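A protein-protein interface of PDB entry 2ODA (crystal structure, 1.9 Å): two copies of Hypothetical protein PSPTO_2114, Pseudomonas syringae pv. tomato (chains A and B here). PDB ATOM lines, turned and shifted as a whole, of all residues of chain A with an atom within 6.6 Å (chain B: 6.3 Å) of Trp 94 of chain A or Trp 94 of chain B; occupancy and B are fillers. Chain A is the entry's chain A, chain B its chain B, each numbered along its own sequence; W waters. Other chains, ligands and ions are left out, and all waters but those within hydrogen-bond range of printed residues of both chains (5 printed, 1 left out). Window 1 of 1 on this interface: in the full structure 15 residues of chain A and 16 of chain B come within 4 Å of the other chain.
The backbone carbonyl oxygen of Gln 104 of chain A sits at hydrogen-bond distance from the side-chain sulfur of Cys 108 of chain A, at 3.5 Å. The backbone carbonyl oxygen (O) of Leu 97 of chain B is in hydrogen-bond range of the backbone NH (N) of Val 102 of chain B. The side-chain sulfur of Cys 108 of chain B sits close to the backbone carbonyl oxygen of Leu 105 of chain B (3.5 Å).
The backbone NH (N) of Leu 105 of chain A lies within hydrogen-bond range of the backbone carbonyl oxygen (O) of Asn 123 of chain B, 2.7 Å away. The backbone carbonyl oxygen of Ser 103 of chain B lies close to the side-chain amide nitrogen of Asn 123 of chain A, at 3.4 Å. The side-chain amide nitrogen of Gln 104 of chain B is in hydrogen-bond range of the side-chain amide oxygen of Asn 123 of chain A (3.3 Å). The backbone carbonyl oxygen (O) of Asn 123 of chain A is in hydrogen-bond range of the backbone NH (N) of Leu 105 of chain B. The side-chain sulfur (SD) of Met 98 of chain B sits close to the side-chain carboxylate (OD2) of Asp 91 of chain A (3.5 Å).
Asp 91 of chain A touches Met 98 of chain B, and with the chains exchanged Met 98 of chain A touches Asp 91 of chain B. Trp 94 of chain A touches Leu 97 of chain B, and with the chains exchanged Leu 97 of chain A touches Trp 94 of chain B. Trp 94 of chain A touches Leu 105 of chain B, and with the chains exchanged Leu 105 of chain A touches Trp 94 of chain B. Positions printed for both chains: 10, 90, 91, 92, 93, 94, 95, 96, 97, 98, 99, 102, 104, 105, 108, 120, 123, 124, 125 and 126.
Of the printed residues of chain B, Trp 94 of chain A touches Trp 94 (3.5 Å), Leu 97 (3.8 Å), Met 98 (3.7 Å) and Leu 105 (3.99 Å). Of chain A, only Trp 94 (3.5 Å), Leu 97 (3.7 Å), Met 98 (3.5 Å) and Leu 105 (3.9 Å) come within 4 Å of Trp 94 of chain B. Of the printed residues of chain A, Val 102 of chain B touches Pro 90 (3.5 Å). Printed residues of chain B within 4 Å of Pro 90 of chain A: Val 102 (3.5 Å) and Ser 103 (3.6 Å). Of the printed residues of chain A, Met 95 of chain B touches Met 98. Ser 120 of chain B touches none of the printed residues of chain A. Cys 108 of chain A touches none of the printed residues of chain B. The nearest printed residue of chain B that does not touch Ala 124 of chain A is Trp 94 of chain B (5.3 Å).
Hydrophobic or aromatic side chains of chain B that line the printed part of chain A: Pro 90, Trp 94, Met 95, Leu 97, Met 98 and Leu 105. Hydrophobic or aromatic side chains of chain A that line the printed part of chain B: Pro 90, Trp 94, Leu 97, Met 98 and Leu 105.
Water W3 lies within hydrogen-bond range of OD1 of Asp 91 of chain B (2.7 Å) and O of Val 102 of chain A (3.3 Å). Water W4 bridges the side-chain carboxylate of Asp 91 of chain A (2.7 Å) and the backbone carbonyl oxygen of Met 98 of chain B (2.8 Å). Water W2 lies within hydrogen-bond range of OD1 of Asp 91 of chain A (2.7 Å) and O of Val 102 of chain B (2.9 Å).
Among the printed residues, merely in contact across the chains: Pro 90 of chain A with Val 102 of chain B (3.5 Å), Pro 90 of chain A with Ser 103 of chain B (3.6 Å), Trp 94 of chain A with Trp 94 of chain B (3.5 Å), Trp 94 of chain A with Leu 97 of chain B (3.8 Å), Trp 94 of chain A with Met 98 of chain B (3.7 Å), Trp 94 of chain A with Leu 105 of chain B (3.99 Å), Leu 97 of chain A with Trp 94 of chain B (3.7 Å), Met 98 of chain A with Asp 91 of chain B (3.2 Å), Met 98 of chain A with Trp 94 of chain B (3.5 Å), Met 98 of chain A with Met 95 of chain B (3.5 Å), Val 102 of chain A with Pro 90 of chain B (3.7 Å), Gln 104 of chain A with Asn 123 of chain B (3.3 Å), Leu 105 of chain A with Trp 94 of chain B (3.9 Å), Leu 105 of chain A with Leu 105 of chain B (3.4 Å), Leu 105 of chain A with Ala 124 of chain B (3.7 Å) and Ala 124 of chain A with Leu 105 of chain B (3.6 Å).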
ATOM      1  N   LEU A  10      -1.888  15.195  -1.423  1.00  0.00           N
ATOM      2  CA  LEU A  10      -2.402  16.556  -1.483  1.00  0.00           C
ATOM      3  C   LEU A  10      -1.338  17.404  -2.134  1.00  0.00           C
ATOM      4  O   LEU A  10      -0.167  17.230  -1.836  1.00  0.00           O
ATOM      5  CB  LEU A  10      -2.683  17.080  -0.073  1.00  0.00           C
ATOM      6  CG  LEU A  10      -3.660  16.247   0.762  1.00  0.00           C
ATOM      7  CD1 LEU A  10      -3.898  16.894   2.154  1.00  0.00           C
ATOM      8  CD2 LEU A  10      -4.958  16.021  -0.031  1.00  0.00           C
ATOM      9  N   PRO A  90      -4.115  23.220  10.795  1.00  0.00           N
ATOM     10  CA  PRO A  90      -4.109  21.923  10.110  1.00  0.00           C
ATOM     11  C   PRO A  90      -5.363  21.695   9.261  1.00  0.00           C
ATOM     12  O   PRO A  90      -5.402  20.755   8.430  1.00  0.00           O
ATOM     13  CB  PRO A  90      -4.074  20.914  11.272  1.00  0.00           C
ATOM     14  CG  PRO A  90      -4.718  21.619  12.415  1.00  0.00           C
ATOM     15  CD  PRO A  90      -4.348  23.083  12.245  1.00  0.00           C
ATOM     16  N   ASP A  91      -6.379  22.534   9.492  1.00  0.00           N
ATOM     17  CA  ASP A  91      -7.723  22.349   8.945  1.00  0.00           C
ATOM     18  C   ASP A  91      -7.766  22.063   7.461  1.00  0.00           C
ATOM     19  O   ASP A  91      -8.467  21.171   7.030  1.00  0.00           O
ATOM     20  CB  ASP A  91      -8.587  23.595   9.212  1.00  0.00           C
ATOM     21  CG  ASP A  91      -8.775  23.873  10.687  1.00  0.00           C
ATOM     22  OD1 ASP A  91      -7.793  23.764  11.466  1.00  0.00           O
ATOM     23  OD2 ASP A  91      -9.904  24.219  11.080  1.00  0.00           O
ATOM     24  N   ALA A  92      -7.047  22.861   6.672  1.00  0.00           N
ATOM     25  CA  ALA A  92      -7.043  22.692   5.203  1.00  0.00           C
ATOM     26  C   ALA A  92      -6.710  21.250   4.818  1.00  0.00           C
ATOM     27  O   ALA A  92      -7.340  20.666   3.916  1.00  0.00           O
ATOM     28  CB  ALA A  92      -6.008  23.660   4.572  1.00  0.00           C
ATOM     29  N   CYS A  93      -5.695  20.694   5.473  1.00  0.00           N
ATOM     30  CA  CYS A  93      -5.247  19.322   5.152  1.00  0.00           C
ATOM     31  C   CYS A  93      -6.252  18.257   5.626  1.00  0.00           C
ATOM     32  O   CYS A  93      -6.598  17.324   4.879  1.00  0.00           O
ATOM     33  CB  CYS A  93      -3.841  19.086   5.708  1.00  0.00           C
ATOM     34  SG  CYS A  93      -2.634  20.098   4.795  1.00  0.00           S
ATOM     35  N   TRP A  94      -6.747  18.394   6.853  1.00  0.00           N
ATOM     36  CA  TRP A  94      -7.801  17.471   7.302  1.00  0.00           C
ATOM     37  C   TRP A  94      -9.042  17.530   6.414  1.00  0.00           C
ATOM     38  O   TRP A  94      -9.624  16.499   6.040  1.00  0.00           O
ATOM     39  CB  TRP A  94      -8.172  17.718   8.759  1.00  0.00           C
ATOM     40  CG  TRP A  94      -7.067  17.408   9.744  1.00  0.00           C
ATOM     41  CD1 TRP A  94      -6.055  16.479   9.594  1.00  0.00           C
ATOM     42  CD2 TRP A  94      -6.896  17.980  11.043  1.00  0.00           C
ATOM     43  NE1 TRP A  94      -5.262  16.470  10.717  1.00  0.00           N
ATOM     44  CE2 TRP A  94      -5.754  17.371  11.624  1.00  0.00           C
ATOM     45  CE3 TRP A  94      -7.586  18.960  11.775  1.00  0.00           C
ATOM     46  CZ2 TRP A  94      -5.295  17.704  12.898  1.00  0.00           C
ATOM     47  CZ3 TRP A  94      -7.128  19.290  13.046  1.00  0.00           C
ATOM     48  CH2 TRP A  94      -5.983  18.662  13.590  1.00  0.00           C
ATOM     49  N   MET A  95      -9.448  18.729   6.036  1.00  0.00           N
ATOM     50  CA  MET A  95     -10.627  18.820   5.199  1.00  0.00           C
ATOM     51  C   MET A  95     -10.439  18.254   3.795  1.00  0.00           C
ATOM     52  O   MET A  95     -11.382  17.692   3.239  1.00  0.00           O
ATOM     53  CB  MET A  95     -11.185  20.232   5.211  1.00  0.00           C
ATOM     54  CG  MET A  95     -12.050  20.436   6.460  1.00  0.00           C
ATOM     55  SD  MET A  95     -12.418  22.310   6.697  1.00  0.00           S
ATOM     56  CE  MET A  95     -13.396  22.608   5.023  1.00  0.00           C
ATOM     57  N   ALA A  96      -9.222  18.374   3.249  1.00  0.00           N
ATOM     58  CA  ALA A  96      -8.856  17.734   1.983  1.00  0.00           C
ATOM     59  C   ALA A  96      -8.958  16.204   2.050  1.00  0.00           C
ATOM     60  O   ALA A  96      -9.610  15.552   1.215  1.00  0.00           O
ATOM     61  CB  ALA A  96      -7.456  18.172   1.589  1.00  0.00           C
ATOM     62  N   LEU A  97      -8.342  15.631   3.075  1.00  0.00           N
ATOM     63  CA  LEU A  97      -8.377  14.182   3.309  1.00  0.00           C
ATOM     64  C   LEU A  97      -9.794  13.695   3.509  1.00  0.00           C
ATOM     65  O   LEU A  97     -10.163  12.653   2.986  1.00  0.00           O
ATOM     66  CB  LEU A  97      -7.524  13.833   4.525  1.00  0.00           C
ATOM     67  CG  LEU A  97      -6.029  14.144   4.405  1.00  0.00           C
ATOM     68  CD1 LEU A  97      -5.353  13.591   5.657  1.00  0.00           C
ATOM     69  CD2 LEU A  97      -5.426  13.476   3.137  1.00  0.00           C
ATOM     70  N   MET A  98     -10.598  14.471   4.246  1.00  0.00           N
ATOM     71  CA  MET A  98     -12.021  14.139   4.409  1.00  0.00           C
ATOM     72  C   MET A  98     -12.803  14.164   3.090  1.00  0.00           C
ATOM     73  O   MET A  98     -13.599  13.255   2.812  1.00  0.00           O
ATOM     74  CB  MET A  98     -12.657  15.052   5.440  1.00  0.00           C
ATOM     75  CG  MET A  98     -12.191  14.754   6.854  1.00  0.00           C
ATOM     76  SD  MET A  98     -12.720  16.178   8.109  1.00  0.00           S
ATOM     77  CE  MET A  98     -14.611  16.169   7.873  1.00  0.00           C
ATOM     78  N   ALA A  99     -12.553  15.171   2.251  1.00  0.00           N
ATOM     79  CA  ALA A  99     -13.211  15.221   0.932  1.00  0.00           C
ATOM     80  C   ALA A  99     -12.834  14.031   0.041  1.00  0.00           C
ATOM     81  O   ALA A  99     -13.588  13.663  -0.873  1.00  0.00           O
ATOM     82  CB  ALA A  99     -12.911  16.543   0.221  1.00  0.00           C
ATOM     83  N   VAL A 102     -10.526   9.441   2.821  1.00  0.00           N
ATOM     84  CA  VAL A 102      -9.430   8.544   3.198  1.00  0.00           C
ATOM     85  C   VAL A 102      -9.805   7.777   4.462  1.00  0.00           C
ATOM     86  O   VAL A 102     -10.534   8.297   5.315  1.00  0.00           O
ATOM     87  CB  VAL A 102      -8.068   9.264   3.360  1.00  0.00           C
ATOM     88  CG1 VAL A 102      -7.785  10.207   2.144  1.00  0.00           C
ATOM     89  CG2 VAL A 102      -7.998  10.001   4.685  1.00  0.00           C
ATOM     90  N   GLN A 104      -7.668   6.582   6.718  1.00  0.00           N
ATOM     91  CA  GLN A 104      -6.732   6.858   7.800  1.00  0.00           C
ATOM     92  C   GLN A 104      -5.686   7.869   7.373  1.00  0.00           C
ATOM     93  O   GLN A 104      -5.394   8.021   6.176  1.00  0.00           O
ATOM     94  CB  GLN A 104      -6.070   5.578   8.279  1.00  0.00           C
ATOM     95  CG  GLN A 104      -5.046   5.083   7.338  1.00  0.00           C
ATOM     96  CD  GLN A 104      -5.126   3.611   7.121  1.00  0.00           C
ATOM     97  OE1 GLN A 104      -4.117   2.910   7.246  1.00  0.00           O
ATOM     98  NE2 GLN A 104      -6.328   3.111   6.790  1.00  0.00           N
ATOM     99  N   LEU A 105      -5.135   8.561   8.363  1.00  0.00           N
ATOM    100  CA  LEU A 105      -4.114   9.572   8.125  1.00  0.00           C
ATOM    101  C   LEU A 105      -2.813   8.922   7.667  1.00  0.00           C
ATOM    102  O   LEU A 105      -2.081   9.491   6.834  1.00  0.00           O
ATOM    103  CB  LEU A 105      -3.857  10.367   9.411  1.00  0.00           C
ATOM    104  CG  LEU A 105      -2.743  11.418   9.361  1.00  0.00           C
ATOM    105  CD1 LEU A 105      -3.212  12.576   8.505  1.00  0.00           C
ATOM    106  CD2 LEU A 105      -2.396  11.877  10.776  1.00  0.00           C
ATOM    107  N   CYS A 108      -0.662   9.389   4.295  1.00  0.00           N
ATOM    108  CA  CYS A 108      -1.023  10.576   3.466  1.00  0.00           C
ATOM    109  C   CYS A 108       0.127  11.588   3.387  1.00  0.00           C
ATOM    110  O   CYS A 108       0.865  11.783   4.348  1.00  0.00           O
ATOM    111  CB  CYS A 108      -2.275  11.272   4.017  1.00  0.00           C
ATOM    112  SG  CYS A 108      -3.739  10.233   3.964  1.00  0.00           S
ATOM    113  N   SER A 120       0.912  23.721   7.498  1.00  0.00           N
ATOM    114  CA  SER A 120      -0.444  23.174   7.684  1.00  0.00           C
ATOM    115  C   SER A 120      -0.395  21.638   7.654  1.00  0.00           C
ATOM    116  O   SER A 120      -0.910  20.962   8.560  1.00  0.00           O
ATOM    117  CB  SER A 120      -1.396  23.695   6.599  1.00  0.00           C
ATOM    118  OG  SER A 120      -2.685  23.133   6.749  1.00  0.00           O
ATOM    119  N   ASN A 123       1.547  20.408  10.773  1.00  0.00           N
ATOM    120  CA  ASN A 123       0.586  20.513  11.888  1.00  0.00           C
ATOM    121  C   ASN A 123      -0.505  19.447  11.851  1.00  0.00           C
ATOM    122  O   ASN A 123      -0.897  18.918  12.897  1.00  0.00           O
ATOM    123  CB  ASN A 123      -0.035  21.911  11.916  1.00  0.00           C
ATOM    124  CG  ASN A 123       0.983  23.002  12.319  1.00  0.00           C
ATOM    125  OD1 ASN A 123       2.080  22.700  12.770  1.00  0.00           O
ATOM    126  ND2 ASN A 123       0.612  24.267  12.130  1.00  0.00           N
ATOM    127  N   ALA A 124      -1.007  19.158  10.652  1.00  0.00           N
ATOM    128  CA  ALA A 124      -2.019  18.143  10.452  1.00  0.00           C
ATOM    129  C   ALA A 124      -1.538  16.698  10.640  1.00  0.00           C
ATOM    130  O   ALA A 124      -2.353  15.798  10.708  1.00  0.00           O
ATOM    131  CB  ALA A 124      -2.686  18.314   9.078  1.00  0.00           C
ATOM    132  N   GLY A 125      -0.220  16.481  10.704  1.00  0.00           N
ATOM    133  CA  GLY A 125       0.326  15.135  10.936  1.00  0.00           C
ATOM    134  C   GLY A 125       0.653  14.329   9.690  1.00  0.00           C
ATOM    135  O   GLY A 125       0.908  13.109   9.782  1.00  0.00           O
ATOM    136  N   LEU A 126       0.636  14.991   8.530  1.00  0.00           N
ATOM    137  CA  LEU A 126       1.020  14.336   7.261  1.00  0.00           C
ATOM    138  C   LEU A 126       2.548  14.259   7.044  1.00  0.00           C
ATOM    139  O   LEU A 126       3.344  14.970   7.682  1.00  0.00           O
ATOM    140  CB  LEU A 126       0.338  14.990   6.030  1.00  0.00           C
ATOM    141  CG  LEU A 126      -1.191  14.861   5.823  1.00  0.00           C
ATOM    142  CD1 LEU A 126      -1.915  15.787   6.758  1.00  0.00           C
ATOM    143  CD2 LEU A 126      -1.582  15.212   4.382  1.00  0.00           C
ATOM    144  N   LEU B  10     -10.055  14.621  23.616  1.00  0.00           N
ATOM    145  CA  LEU B  10     -11.376  14.255  23.086  1.00  0.00           C
ATOM    146  C   LEU B  10     -11.930  13.117  23.902  1.00  0.00           C
ATOM    147  O   LEU B  10     -11.185  12.190  24.222  1.00  0.00           O
ATOM    148  CB  LEU B  10     -11.247  13.806  21.634  1.00  0.00           C
ATOM    149  CG  LEU B  10     -10.553  14.817  20.711  1.00  0.00           C
ATOM    150  CD1 LEU B  10     -10.531  14.246  19.283  1.00  0.00           C
ATOM    151  CD2 LEU B  10     -11.241  16.203  20.755  1.00  0.00           C
ATOM    152  N   PRO B  90     -11.965   9.016  10.173  1.00  0.00           N
ATOM    153  CA  PRO B  90     -11.277   9.947  11.098  1.00  0.00           C
ATOM    154  C   PRO B  90     -12.027  11.272  11.346  1.00  0.00           C
ATOM    155  O   PRO B  90     -11.718  11.998  12.318  1.00  0.00           O
ATOM    156  CB  PRO B  90      -9.946  10.251  10.370  1.00  0.00           C
ATOM    157  CG  PRO B  90     -10.259   9.964   8.887  1.00  0.00           C
ATOM    158  CD  PRO B  90     -11.175   8.765   8.953  1.00  0.00           C
ATOM    159  N   ASP B  91     -12.984  11.576  10.464  1.00  0.00           N
ATOM    160  CA  ASP B  91     -13.728  12.852  10.452  1.00  0.00           C
ATOM    161  C   ASP B  91     -14.226  13.337  11.824  1.00  0.00           C
ATOM    162  O   ASP B  91     -14.041  14.494  12.170  1.00  0.00           O
ATOM    163  CB  ASP B  91     -14.932  12.763   9.520  1.00  0.00           C
ATOM    164  CG  ASP B  91     -14.551  12.437   8.097  1.00  0.00           C
ATOM    165  OD1 ASP B  91     -13.683  11.565   7.882  1.00  0.00           O
ATOM    166  OD2 ASP B  91     -15.136  13.068   7.197  1.00  0.00           O
ATOM    167  N   ALA B  92     -14.882  12.461  12.584  1.00  0.00           N
ATOM    168  CA  ALA B  92     -15.399  12.853  13.885  1.00  0.00           C
ATOM    169  C   ALA B  92     -14.295  13.457  14.780  1.00  0.00           C
ATOM    170  O   ALA B  92     -14.526  14.432  15.491  1.00  0.00           O
ATOM    171  CB  ALA B  92     -16.043  11.679  14.564  1.00  0.00           C
ATOM    172  N   CYS B  93     -13.101  12.871  14.742  1.00  0.00           N
ATOM    173  CA  CYS B  93     -11.994  13.347  15.585  1.00  0.00           C
ATOM    174  C   CYS B  93     -11.347  14.624  15.043  1.00  0.00           C
ATOM    175  O   CYS B  93     -11.084  15.576  15.798  1.00  0.00           O
ATOM    176  CB  CYS B  93     -10.956  12.247  15.745  1.00  0.00           C
ATOM    177  SG  CYS B  93     -11.602  10.849  16.728  1.00  0.00           S
ATOM    178  N   TRP B  94     -11.111  14.660  13.733  1.00  0.00           N
ATOM    179  CA  TRP B  94     -10.584  15.881  13.137  1.00  0.00           C
ATOM    180  C   TRP B  94     -11.523  17.051  13.320  1.00  0.00           C
ATOM    181  O   TRP B  94     -11.089  18.163  13.653  1.00  0.00           O
ATOM    182  CB  TRP B  94     -10.294  15.671  11.661  1.00  0.00           C
ATOM    183  CG  TRP B  94      -9.115  14.782  11.417  1.00  0.00           C
ATOM    184  CD1 TRP B  94      -8.060  14.533  12.264  1.00  0.00           C
ATOM    185  CD2 TRP B  94      -8.843  14.066  10.212  1.00  0.00           C
ATOM    186  NE1 TRP B  94      -7.157  13.673  11.647  1.00  0.00           N
ATOM    187  CE2 TRP B  94      -7.622  13.376  10.392  1.00  0.00           C
ATOM    188  CE3 TRP B  94      -9.528  13.917   9.003  1.00  0.00           C
ATOM    189  CZ2 TRP B  94      -7.055  12.567   9.382  1.00  0.00           C
ATOM    190  CZ3 TRP B  94      -8.962  13.113   7.996  1.00  0.00           C
ATOM    191  CH2 TRP B  94      -7.756  12.433   8.206  1.00  0.00           C
ATOM    192  N   MET B  95     -12.820  16.808  13.134  1.00  0.00           N
ATOM    193  CA  MET B  95     -13.778  17.884  13.319  1.00  0.00           C
ATOM    194  C   MET B  95     -13.843  18.414  14.743  1.00  0.00           C
ATOM    195  O   MET B  95     -13.990  19.608  14.944  1.00  0.00           O
ATOM    196  CB  MET B  95     -15.142  17.505  12.774  1.00  0.00           C
ATOM    197  CG  MET B  95     -15.179  17.744  11.301  1.00  0.00           C
ATOM    198  SD  MET B  95     -16.783  16.990  10.540  1.00  0.00           S
ATOM    199  CE  MET B  95     -18.060  18.097  11.449  1.00  0.00           C
ATOM    200  N   ALA B  96     -13.685  17.526  15.720  1.00  0.00           N
ATOM    201  CA  ALA B  96     -13.612  17.908  17.115  1.00  0.00           C
ATOM    202  C   ALA B  96     -12.379  18.752  17.381  1.00  0.00           C
ATOM    203  O   ALA B  96     -12.454  19.769  18.085  1.00  0.00           O
ATOM    204  CB  ALA B  96     -13.579  16.669  17.986  1.00  0.00           C
ATOM    205  N   LEU B  97     -11.227  18.328  16.857  1.00  0.00           N
ATOM    206  CA  LEU B  97      -9.998  19.135  17.024  1.00  0.00           C
ATOM    207  C   LEU B  97     -10.150  20.543  16.419  1.00  0.00           C
ATOM    208  O   LEU B  97      -9.744  21.549  17.015  1.00  0.00           O
ATOM    209  CB  LEU B  97      -8.769  18.389  16.468  1.00  0.00           C
ATOM    210  CG  LEU B  97      -8.418  17.037  17.110  1.00  0.00           C
ATOM    211  CD1 LEU B  97      -7.246  16.399  16.346  1.00  0.00           C
ATOM    212  CD2 LEU B  97      -8.093  17.220  18.623  1.00  0.00           C
ATOM    213  N   MET B  98     -10.736  20.621  15.229  1.00  0.00           N
ATOM    214  CA  MET B  98     -11.011  21.916  14.598  1.00  0.00           C
ATOM    215  C   MET B  98     -11.927  22.815  15.414  1.00  0.00           C
ATOM    216  O   MET B  98     -11.698  24.031  15.504  1.00  0.00           O
ATOM    217  CB  MET B  98     -11.547  21.717  13.184  1.00  0.00           C
ATOM    218  CG  MET B  98     -10.454  21.184  12.263  1.00  0.00           C
ATOM    219  SD  MET B  98     -11.135  20.971  10.450  1.00  0.00           S
ATOM    220  CE  MET B  98     -11.707  19.196  10.532  1.00  0.00           C
ATOM    221  N   ALA B  99     -12.938  22.210  16.033  1.00  0.00           N
ATOM    222  CA  ALA B  99     -13.859  22.915  16.929  1.00  0.00           C
ATOM    223  C   ALA B  99     -13.135  23.500  18.134  1.00  0.00           C
ATOM    224  O   ALA B  99     -13.586  24.491  18.699  1.00  0.00           O
ATOM    225  CB  ALA B  99     -14.998  21.981  17.378  1.00  0.00           C
ATOM    226  N   VAL B 102      -7.445  23.590  17.515  1.00  0.00           N
ATOM    227  CA  VAL B 102      -6.169  22.936  17.765  1.00  0.00           C
ATOM    228  C   VAL B 102      -5.162  23.322  16.679  1.00  0.00           C
ATOM    229  O   VAL B 102      -5.499  23.352  15.496  1.00  0.00           O
ATOM    230  CB  VAL B 102      -6.388  21.396  17.867  1.00  0.00           C
ATOM    231  CG1 VAL B 102      -5.144  20.605  17.569  1.00  0.00           C
ATOM    232  CG2 VAL B 102      -6.946  21.037  19.269  1.00  0.00           C
ATOM    233  N   SER B 103      -3.937  23.624  17.082  1.00  0.00           N
ATOM    234  CA  SER B 103      -2.939  24.046  16.097  1.00  0.00           C
ATOM    235  C   SER B 103      -2.080  22.890  15.557  1.00  0.00           C
ATOM    236  O   SER B 103      -1.480  23.013  14.483  1.00  0.00           O
ATOM    237  CB  SER B 103      -2.078  25.183  16.657  1.00  0.00           C
ATOM    238  OG  SER B 103      -1.219  24.701  17.690  1.00  0.00           O
ATOM    239  N   GLN B 104      -1.985  21.791  16.313  1.00  0.00           N
ATOM    240  CA  GLN B 104      -1.218  20.612  15.887  1.00  0.00           C
ATOM    241  C   GLN B 104      -1.882  19.317  16.357  1.00  0.00           C
ATOM    242  O   GLN B 104      -2.340  19.231  17.507  1.00  0.00           O
ATOM    243  CB  GLN B 104       0.205  20.611  16.475  1.00  0.00           C
ATOM    244  CG  GLN B 104       1.186  21.574  15.855  1.00  0.00           C
ATOM    245  CD  GLN B 104       1.169  22.945  16.517  1.00  0.00           C
ATOM    246  OE1 GLN B 104       0.708  23.087  17.648  1.00  0.00           O
ATOM    247  NE2 GLN B 104       1.685  23.960  15.818  1.00  0.00           N
ATOM    248  N   LEU B 105      -1.883  18.301  15.486  1.00  0.00           N
ATOM    249  CA  LEU B 105      -2.285  16.950  15.886  1.00  0.00           C
ATOM    250  C   LEU B 105      -1.418  16.396  17.020  1.00  0.00           C
ATOM    251  O   LEU B 105      -1.905  15.648  17.898  1.00  0.00           O
ATOM    252  CB  LEU B 105      -2.158  16.000  14.676  1.00  0.00           C
ATOM    253  CG  LEU B 105      -2.578  14.543  14.868  1.00  0.00           C
ATOM    254  CD1 LEU B 105      -4.068  14.455  15.221  1.00  0.00           C
ATOM    255  CD2 LEU B 105      -2.300  13.731  13.633  1.00  0.00           C
ATOM    256  N   CYS B 108      -2.413  15.212  20.794  1.00  0.00           N
ATOM    257  CA  CYS B 108      -3.868  15.110  21.032  1.00  0.00           C
ATOM    258  C   CYS B 108      -4.266  13.674  21.401  1.00  0.00           C
ATOM    259  O   CYS B 108      -3.701  12.716  20.873  1.00  0.00           O
ATOM    260  CB  CYS B 108      -4.660  15.602  19.822  1.00  0.00           C
ATOM    261  SG  CYS B 108      -4.472  17.376  19.510  1.00  0.00           S
ATOM    262  N   SER B 120     -11.808   5.303  14.998  1.00  0.00           N
ATOM    263  CA  SER B 120     -11.790   6.643  14.387  1.00  0.00           C
ATOM    264  C   SER B 120     -10.554   7.423  14.878  1.00  0.00           C
ATOM    265  O   SER B 120      -9.863   8.054  14.087  1.00  0.00           O
ATOM    266  CB  SER B 120     -13.096   7.400  14.702  1.00  0.00           C
ATOM    267  OG  SER B 120     -13.011   8.765  14.311  1.00  0.00           O
ATOM    268  N   ASN B 123      -7.401   5.993  13.375  1.00  0.00           N
ATOM    269  CA  ASN B 123      -7.390   6.413  11.956  1.00  0.00           C
ATOM    270  C   ASN B 123      -7.053   7.886  11.776  1.00  0.00           C
ATOM    271  O   ASN B 123      -6.401   8.285  10.780  1.00  0.00           O
ATOM    272  CB  ASN B 123      -8.739   6.103  11.302  1.00  0.00           C
ATOM    273  CG  ASN B 123      -8.949   4.594  11.070  1.00  0.00           C
ATOM    274  OD1 ASN B 123      -7.998   3.827  11.124  1.00  0.00           O
ATOM    275  ND2 ASN B 123     -10.203   4.175  10.836  1.00  0.00           N
ATOM    276  N   ALA B 124      -7.478   8.704  12.734  1.00  0.00           N
ATOM    277  CA  ALA B 124      -7.240  10.154  12.663  1.00  0.00           C
ATOM    278  C   ALA B 124      -5.809  10.520  13.102  1.00  0.00           C
ATOM    279  O   ALA B 124      -5.379  11.673  12.963  1.00  0.00           O
ATOM    280  CB  ALA B 124      -8.287  10.905  13.519  1.00  0.00           C
ATOM    281  N   GLY B 125      -5.078   9.538  13.622  1.00  0.00           N
ATOM    282  CA  GLY B 125      -3.676   9.752  13.975  1.00  0.00           C
ATOM    283  C   GLY B 125      -3.452  10.135  15.426  1.00  0.00           C
ATOM    284  O   GLY B 125      -2.354  10.568  15.782  1.00  0.00           O
ATOM    285  N   LEU B 126      -4.493   9.994  16.259  1.00  0.00           N
ATOM    286  CA  LEU B 126      -4.398  10.388  17.675  1.00  0.00           C
ATOM    287  C   LEU B 126      -3.809   9.306  18.578  1.00  0.00           C
ATOM    288  O   LEU B 126      -3.765   8.121  18.222  1.00  0.00           O
ATOM    289  CB  LEU B 126      -5.782  10.800  18.223  1.00  0.00           C
ATOM    290  CG  LEU B 126      -6.231  12.228  17.845  1.00  0.00           C
ATOM    291  CD1 LEU B 126      -6.833  12.239  16.455  1.00  0.00           C
ATOM    292  CD2 LEU B 126      -7.253  12.789  18.843  1.00  0.00           C
HETATM  293  O   HOH W   1     -15.766  12.939   4.620  1.00  0.00           O
HETATM  294  O   HOH W   2      -8.090  23.644  14.158  1.00  0.00           O
HETATM  295  O   HOH W   3     -13.055  10.430   5.509  1.00  0.00           O
HETATM  296  O   HOH W   4     -10.584  25.490  13.376  1.00  0.00           O
HETATM  297  O   HOH W   5      -3.717   6.750  10.898  1.00  0.00           O
